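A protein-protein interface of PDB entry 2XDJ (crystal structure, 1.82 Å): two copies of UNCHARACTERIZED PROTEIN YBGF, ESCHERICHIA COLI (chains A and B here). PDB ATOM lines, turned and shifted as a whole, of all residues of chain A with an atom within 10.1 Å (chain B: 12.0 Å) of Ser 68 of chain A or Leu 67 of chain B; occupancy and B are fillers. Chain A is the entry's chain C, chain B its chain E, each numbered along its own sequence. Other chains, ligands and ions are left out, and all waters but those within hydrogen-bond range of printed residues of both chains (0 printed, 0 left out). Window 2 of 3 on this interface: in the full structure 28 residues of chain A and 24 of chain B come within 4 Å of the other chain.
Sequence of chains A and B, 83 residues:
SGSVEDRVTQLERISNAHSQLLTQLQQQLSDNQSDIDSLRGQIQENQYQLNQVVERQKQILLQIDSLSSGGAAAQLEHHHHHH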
ATOM      1  N   ILE A  60       3.693 -16.273  26.036  1.00  0.00           N
ATOM      2  CA  ILE A  60       2.253 -16.496  25.804  1.00  0.00           C
ATOM      3  C   ILE A  60       1.486 -16.137  27.098  1.00  0.00           C
ATOM      4  O   ILE A  60       0.514 -15.364  27.080  1.00  0.00           O
ATOM      5  CB  ILE A  60       1.913 -17.926  25.318  1.00  0.00           C
ATOM      6  CG1 ILE A  60       2.366 -18.129  23.847  1.00  0.00           C
ATOM      7  CG2 ILE A  60       0.364 -18.213  25.411  1.00  0.00           C
ATOM      8  CD1 ILE A  60       2.492 -19.652  23.416  1.00  0.00           C
ATOM      9  N   LEU A  61       2.024 -16.615  28.217  1.00  0.00           N
ATOM     10  CA  LEU A  61       1.385 -16.360  29.542  1.00  0.00           C
ATOM     11  C   LEU A  61       1.327 -14.873  29.805  1.00  0.00           C
ATOM     12  O   LEU A  61       0.281 -14.339  30.170  1.00  0.00           O
ATOM     13  CB  LEU A  61       2.140 -17.092  30.651  1.00  0.00           C
ATOM     14  CG  LEU A  61       2.031 -18.609  30.650  1.00  0.00           C
ATOM     15  CD1 LEU A  61       3.030 -19.261  31.690  1.00  0.00           C
ATOM     16  CD2 LEU A  61       0.648 -19.043  31.001  1.00  0.00           C
ATOM     17  N   LEU A  62       2.422 -14.181  29.512  1.00  0.00           N
ATOM     18  CA  LEU A  62       2.459 -12.720  29.701  1.00  0.00           C
ATOM     19  C   LEU A  62       1.525 -12.015  28.705  1.00  0.00           C
ATOM     20  O   LEU A  62       0.976 -10.980  29.013  1.00  0.00           O
ATOM     21  CB  LEU A  62       3.890 -12.233  29.534  1.00  0.00           C
ATOM     22  CG  LEU A  62       4.817 -12.707  30.703  1.00  0.00           C
ATOM     23  CD1 LEU A  62       6.300 -12.496  30.426  1.00  0.00           C
ATOM     24  CD2 LEU A  62       4.471 -12.071  32.019  1.00  0.00           C
ATOM     25  N   GLN A  63       1.384 -12.579  27.502  1.00  0.00           N
ATOM     26  CA  GLN A  63       0.561 -11.942  26.482  1.00  0.00           C
ATOM     27  C   GLN A  63      -0.908 -12.028  26.938  1.00  0.00           C
ATOM     28  O   GLN A  63      -1.689 -11.090  26.806  1.00  0.00           O
ATOM     29  CB  GLN A  63       0.817 -12.620  25.145  1.00  0.00           C
ATOM     30  CG  GLN A  63      -0.273 -12.427  24.148  1.00  0.00           C
ATOM     31  CD  GLN A  63      -0.113 -11.204  23.312  1.00  0.00           C
ATOM     32  OE1 GLN A  63       0.197 -10.108  23.830  1.00  0.00           O
ATOM     33  NE2 GLN A  63      -0.382 -11.343  22.002  1.00  0.00           N
ATOM     34  N   ILE A  64      -1.264 -13.164  27.514  1.00  0.00           N
ATOM     35  CA  ILE A  64      -2.572 -13.400  28.062  1.00  0.00           C
ATOM     36  C   ILE A  64      -2.849 -12.405  29.207  1.00  0.00           C
ATOM     37  O   ILE A  64      -3.944 -11.846  29.277  1.00  0.00           O
ATOM     38  CB  ILE A  64      -2.668 -14.934  28.539  1.00  0.00           C
ATOM     39  CG1 ILE A  64      -2.782 -15.897  27.336  1.00  0.00           C
ATOM     40  CG2 ILE A  64      -3.782 -15.188  29.611  1.00  0.00           C
ATOM     41  CD1 ILE A  64      -2.778 -17.411  27.776  1.00  0.00           C
ATOM     42  N   ASP A  65      -1.867 -12.180  30.072  1.00  0.00           N
ATOM     43  CA  ASP A  65      -1.978 -11.194  31.160  1.00  0.00           C
ATOM     44  C   ASP A  65      -2.254  -9.783  30.597  1.00  0.00           C
ATOM     45  O   ASP A  65      -3.131  -9.074  31.107  1.00  0.00           O
ATOM     46  CB  ASP A  65      -0.705 -11.203  32.012  1.00  0.00           C
ATOM     47  CG  ASP A  65      -0.564 -12.495  32.793  1.00  0.00           C
ATOM     48  OD1 ASP A  65      -1.613 -13.069  33.183  1.00  0.00           O
ATOM     49  OD2 ASP A  65       0.563 -12.959  32.989  1.00  0.00           O
ATOM     50  N   SER A  66      -1.513  -9.408  29.546  1.00  0.00           N
ATOM     51  CA  SER A  66      -1.701  -8.111  28.881  1.00  0.00           C
ATOM     52  C   SER A  66      -3.077  -8.012  28.289  1.00  0.00           C
ATOM     53  O   SER A  66      -3.727  -6.979  28.485  1.00  0.00           O
ATOM     54  CB  SER A  66      -0.706  -7.908  27.756  1.00  0.00           C
ATOM     55  OG  SER A  66       0.590  -7.888  28.291  1.00  0.00           O
ATOM     56  N   LEU A  67      -3.508  -9.055  27.563  1.00  0.00           N
ATOM     57  CA  LEU A  67      -4.853  -9.117  27.011  1.00  0.00           C
ATOM     58  C   LEU A  67      -5.949  -8.958  28.077  1.00  0.00           C
ATOM     59  O   LEU A  67      -6.980  -8.296  27.839  1.00  0.00           O
ATOM     60  CB  LEU A  67      -5.056 -10.430  26.239  1.00  0.00           C
ATOM     61  CG  LEU A  67      -4.406 -10.511  24.846  1.00  0.00           C
ATOM     62  CD1 LEU A  67      -4.330 -11.955  24.198  1.00  0.00           C
ATOM     63  CD2 LEU A  67      -5.118  -9.521  23.878  1.00  0.00           C
ATOM     64  N   SER A  68      -5.731  -9.586  29.242  1.00  0.00           N
ATOM     65  CA  SER A  68      -6.719  -9.596  30.354  1.00  0.00           C
ATOM     66  C   SER A  68      -7.041  -8.204  30.884  1.00  0.00           C
ATOM     67  O   SER A  68      -8.035  -8.038  31.591  1.00  0.00           O
ATOM     68  CB  SER A  68      -6.196 -10.440  31.547  1.00  0.00           C
ATOM     69  OG  SER A  68      -6.001 -11.811  31.204  1.00  0.00           O
ATOM     70  N   SER A  69      -6.158  -7.244  30.604  1.00  0.00           N
ATOM     71  CA  SER A  69      -6.323  -5.833  30.948  1.00  0.00           C
ATOM     72  C   SER A  69      -6.712  -5.065  29.677  1.00  0.00           C
ATOM     73  O   SER A  69      -6.776  -3.833  29.681  1.00  0.00           O
ATOM     74  CB  SER A  69      -5.025  -5.271  31.538  1.00  0.00           C
ATOM     75  OG  SER A  69      -3.973  -5.404  30.594  1.00  0.00           O
ATOM     76  N   GLN B  57       0.132 -26.216  28.689  1.00  0.00           N
ATOM     77  CA  GLN B  57      -0.638 -25.867  27.452  1.00  0.00           C
ATOM     78  C   GLN B  57      -2.142 -25.974  27.638  1.00  0.00           C
ATOM     79  O   GLN B  57      -2.893 -25.117  27.135  1.00  0.00           O
ATOM     80  CB  GLN B  57      -0.195 -26.753  26.306  1.00  0.00           C
ATOM     81  CG  GLN B  57       1.159 -26.395  25.865  1.00  0.00           C
ATOM     82  CD  GLN B  57       1.567 -27.149  24.598  1.00  0.00           C
ATOM     83  OE1 GLN B  57       1.947 -26.542  23.583  1.00  0.00           O
ATOM     84  NE2 GLN B  57       1.492 -28.481  24.652  1.00  0.00           N
ATOM     85  N   LYS B  58      -2.584 -27.007  28.368  1.00  0.00           N
ATOM     86  CA  LYS B  58      -4.008 -27.131  28.723  1.00  0.00           C
ATOM     87  C   LYS B  58      -4.464 -25.955  29.554  1.00  0.00           C
ATOM     88  O   LYS B  58      -5.563 -25.453  29.356  1.00  0.00           O
ATOM     89  CB  LYS B  58      -4.303 -28.407  29.544  1.00  0.00           C
ATOM     90  CG  LYS B  58      -4.026 -29.698  28.806  1.00  0.00           C
ATOM     91  CD  LYS B  58      -4.419 -30.964  29.609  1.00  0.00           C
ATOM     92  CE  LYS B  58      -3.592 -32.174  29.126  1.00  0.00           C
ATOM     93  NZ  LYS B  58      -4.395 -33.460  29.415  1.00  0.00           N
ATOM     94  N   GLN B  59      -3.657 -25.530  30.517  1.00  0.00           N
ATOM     95  CA  GLN B  59      -4.039 -24.355  31.301  1.00  0.00           C
ATOM     96  C   GLN B  59      -4.069 -23.064  30.441  1.00  0.00           C
ATOM     97  O   GLN B  59      -4.937 -22.223  30.656  1.00  0.00           O
ATOM     98  CB  GLN B  59      -3.069 -24.156  32.469  1.00  0.00           C
ATOM     99  CG  GLN B  59      -3.154 -25.326  33.455  1.00  0.00           C
ATOM    100  CD  GLN B  59      -2.114 -25.207  34.587  1.00  0.00           C
ATOM    101  OE1 GLN B  59      -1.212 -24.394  34.476  1.00  0.00           O
ATOM    102  NE2 GLN B  59      -2.230 -26.061  35.651  1.00  0.00           N
ATOM    103  N   ILE B  60      -3.099 -22.908  29.537  1.00  0.00           N
ATOM    104  CA  ILE B  60      -3.076 -21.748  28.616  1.00  0.00           C
ATOM    105  C   ILE B  60      -4.366 -21.697  27.752  1.00  0.00           C
ATOM    106  O   ILE B  60      -4.995 -20.621  27.602  1.00  0.00           O
ATOM    107  CB  ILE B  60      -1.822 -21.832  27.748  1.00  0.00           C
ATOM    108  CG1 ILE B  60      -0.624 -21.402  28.584  1.00  0.00           C
ATOM    109  CG2 ILE B  60      -1.950 -20.952  26.518  1.00  0.00           C
ATOM    110  CD1 ILE B  60       0.697 -21.839  28.064  1.00  0.00           C
ATOM    111  N   LEU B  61      -4.794 -22.861  27.275  1.00  0.00           N
ATOM    112  CA  LEU B  61      -6.038 -22.968  26.462  1.00  0.00           C
ATOM    113  C   LEU B  61      -7.234 -22.509  27.247  1.00  0.00           C
ATOM    114  O   LEU B  61      -8.035 -21.709  26.733  1.00  0.00           O
ATOM    115  CB  LEU B  61      -6.220 -24.396  25.875  1.00  0.00           C
ATOM    116  CG  LEU B  61      -5.432 -24.545  24.580  1.00  0.00           C
ATOM    117  CD1 LEU B  61      -5.142 -26.028  24.246  1.00  0.00           C
ATOM    118  CD2 LEU B  61      -6.254 -23.752  23.474  1.00  0.00           C
ATOM    119  N   LEU B  62      -7.362 -22.924  28.512  1.00  0.00           N
ATOM    120  CA  LEU B  62      -8.459 -22.459  29.304  1.00  0.00           C
ATOM    121  C   LEU B  62      -8.371 -20.953  29.525  1.00  0.00           C
ATOM    122  O   LEU B  62      -9.402 -20.250  29.539  1.00  0.00           O
ATOM    123  CB  LEU B  62      -8.484 -23.153  30.667  1.00  0.00           C
ATOM    124  CG  LEU B  62      -8.675 -24.668  30.725  1.00  0.00           C
ATOM    125  CD1 LEU B  62      -8.520 -25.113  32.188  1.00  0.00           C
ATOM    126  CD2 LEU B  62     -10.070 -25.081  30.083  1.00  0.00           C
ATOM    127  N   GLN B  63      -7.158 -20.420  29.702  1.00  0.00           N
ATOM    128  CA  GLN B  63      -7.070 -19.006  29.960  1.00  0.00           C
ATOM    129  C   GLN B  63      -7.473 -18.186  28.697  1.00  0.00           C
ATOM    130  O   GLN B  63      -8.147 -17.120  28.778  1.00  0.00           O
ATOM    131  CB  GLN B  63      -5.648 -18.659  30.442  1.00  0.00           C
ATOM    132  CG  GLN B  63      -5.311 -18.904  31.914  1.00  0.00           C
ATOM    133  CD  GLN B  63      -4.094 -18.049  32.344  1.00  0.00           C
ATOM    134  OE1 GLN B  63      -3.042 -18.152  31.714  1.00  0.00           O
ATOM    135  NE2 GLN B  63      -4.256 -17.158  33.382  1.00  0.00           N
ATOM    136  N   ILE B  64      -7.035 -18.679  27.536  1.00  0.00           N
ATOM    137  CA  ILE B  64      -7.387 -18.140  26.208  1.00  0.00           C
ATOM    138  C   ILE B  64      -8.898 -18.198  26.001  1.00  0.00           C
ATOM    139  O   ILE B  64      -9.510 -17.211  25.520  1.00  0.00           O
ATOM    140  CB  ILE B  64      -6.653 -18.880  25.079  1.00  0.00           C
ATOM    141  CG1 ILE B  64      -5.222 -18.385  24.969  1.00  0.00           C
ATOM    142  CG2 ILE B  64      -7.383 -18.703  23.692  1.00  0.00           C
ATOM    143  CD1 ILE B  64      -4.347 -19.290  24.107  1.00  0.00           C
ATOM    144  N   ASP B  65      -9.505 -19.308  26.416  1.00  0.00           N
ATOM    145  CA  ASP B  65     -10.964 -19.412  26.405  1.00  0.00           C
ATOM    146  C   ASP B  65     -11.663 -18.320  27.194  1.00  0.00           C
ATOM    147  O   ASP B  65     -12.600 -17.726  26.668  1.00  0.00           O
ATOM    148  CB  ASP B  65     -11.439 -20.763  26.887  1.00  0.00           C
ATOM    149  CG  ASP B  65     -10.990 -21.895  25.979  1.00  0.00           C
ATOM    150  OD1 ASP B  65     -10.656 -21.703  24.782  1.00  0.00           O
ATOM    151  OD2 ASP B  65     -10.912 -23.004  26.502  1.00  0.00           O
ATOM    152  N   SER B  66     -11.243 -18.053  28.429  1.00  0.00           N
ATOM    153  CA  SER B  66     -11.846 -16.925  29.184  1.00  0.00           C
ATOM    154  C   SER B  66     -11.775 -15.602  28.433  1.00  0.00           C
ATOM    155  O   SER B  66     -12.732 -14.799  28.479  1.00  0.00           O
ATOM    156  CB  SER B  66     -11.209 -16.722  30.539  1.00  0.00           C
ATOM    157  OG  SER B  66     -11.302 -17.880  31.316  1.00  0.00           O
ATOM    158  N   LEU B  67     -10.668 -15.371  27.726  1.00  0.00           N
ATOM    159  CA  LEU B  67     -10.501 -14.122  26.963  1.00  0.00           C
ATOM    160  C   LEU B  67     -11.568 -13.914  25.865  1.00  0.00           C
ATOM    161  O   LEU B  67     -12.023 -12.795  25.675  1.00  0.00           O
ATOM    162  CB  LEU B  67      -9.062 -13.975  26.433  1.00  0.00           C
ATOM    163  CG  LEU B  67      -7.991 -13.830  27.537  1.00  0.00           C
ATOM    164  CD1 LEU B  67      -6.551 -13.839  26.986  1.00  0.00           C
ATOM    165  CD2 LEU B  67      -8.242 -12.571  28.385  1.00  0.00           C
ATOM    166  N   SER B  68     -11.971 -14.976  25.159  1.00  0.00           N
ATOM    167  CA  SER B  68     -13.233 -14.954  24.376  1.00  0.00           C
ATOM    168  C   SER B  68     -14.353 -15.746  25.067  1.00  0.00           C
ATOM    169  O   SER B  68     -15.222 -15.180  25.737  1.00  0.00           O
ATOM    170  CB  SER B  68     -13.019 -15.496  22.956  1.00  0.00           C
ATOM    171  OG  SER B  68     -12.375 -16.769  22.975  1.00  0.00           O
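O of Ile 64 of chain A sits at hydrogen-bond distance from OG of Ser 68 of chain A, at 2.8 Å.
Ile 60 of chain A touches Ile 60 of chain B. CG1 of Ile 60 of chain B touches CD2 of Leu 61 of chain A, at 3.6 Å. Gln 63 of chain B touches Leu 61 of chain A. Ile 64 of chain A touches Ile 60 of chain B. Gln 63 of chain B touches Ile 64 of chain A (OE1 to CG2, 3.7 Å). Ile 64 of chain B touches Ile 64 of chain A (CG1 to CD1, 3.8 Å). CD1 of Leu 67 of chain B touches CB of Leu 67 of chain A, at 3.8 Å. Ser 68 of chain A touches Leu 67 of chain B.
Of chain B, only Leu 67 (3.7 Å) comes within 4 Å of Ser 68 of chain A. Of the printed residues of chain A, Leu 67 of chain B touches Leu 67 and Ser 68. Ser 66 of chain A touches none of the printed residues of chain B. Leu 67 of chain A touches just one residue of chain B: Leu 67 (3.8 Å). No residue of chain B comes within 4 Å of Ser 69 of chain A. Of the printed residues of chain A, Ile 64 of chain B touches Ile 64 (3.8 Å). Of the printed residues of chain A, Ile 60 of chain B touches Ile 60, Leu 61 and Ile 64. Of the printed residues of chain B, Leu 61 of chain A touches Ile 60 and Gln 63. Leu 62 of chain B touches none of the printed residues of chain A. Asp 65 of chain B touches none of the printed residues of chain A. The nearest residue of chain B that does not touch Ser 68 of chain A is Gln 63 of chain B (6.0 Å).
Of the 10 printed residues of chain A, 5 touch a printed residue of chain B. Printed residues of chain B that touch a printed residue of chain A: Ile 60, Gln 63, Ile 64 and Leu 67. Hydrophobic or aromatic side chains of chain B within 4 Å of the printed part of chain A: Ile 60, Ile 64 and Leu 67. Among the printed residues, no Asp or Glu carboxylate lies within 4 Å of a Lys or Arg side-chain nitrogen of the other chain.
Leu 61 of chain A touches Ile 60 of chain B, but with the chains exchanged Ile 60 of chain A does not touch Leu 61 of chain B (7.2 Å). Leu 61 of chain A touches Gln 63 of chain B, but with the chains exchanged Gln 63 of chain A does not touch Leu 61 of chain B (11.5 Å). Ile 64 of chain A touches Ile 60 of chain B, but with the chains exchanged Ile 60 of chain A does not touch Ile 64 of chain B (5.0 Å). Leu 67 of chain A touches its own counterpart, Leu 67 of chain B. Positions printed for both chains: 60, 61, 62, 63, 64, 65, 66, 67 and 68. Of the 8 pairs that touch across the chains among the printed residues, 3 have their exchanged pair printed and touching as well.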
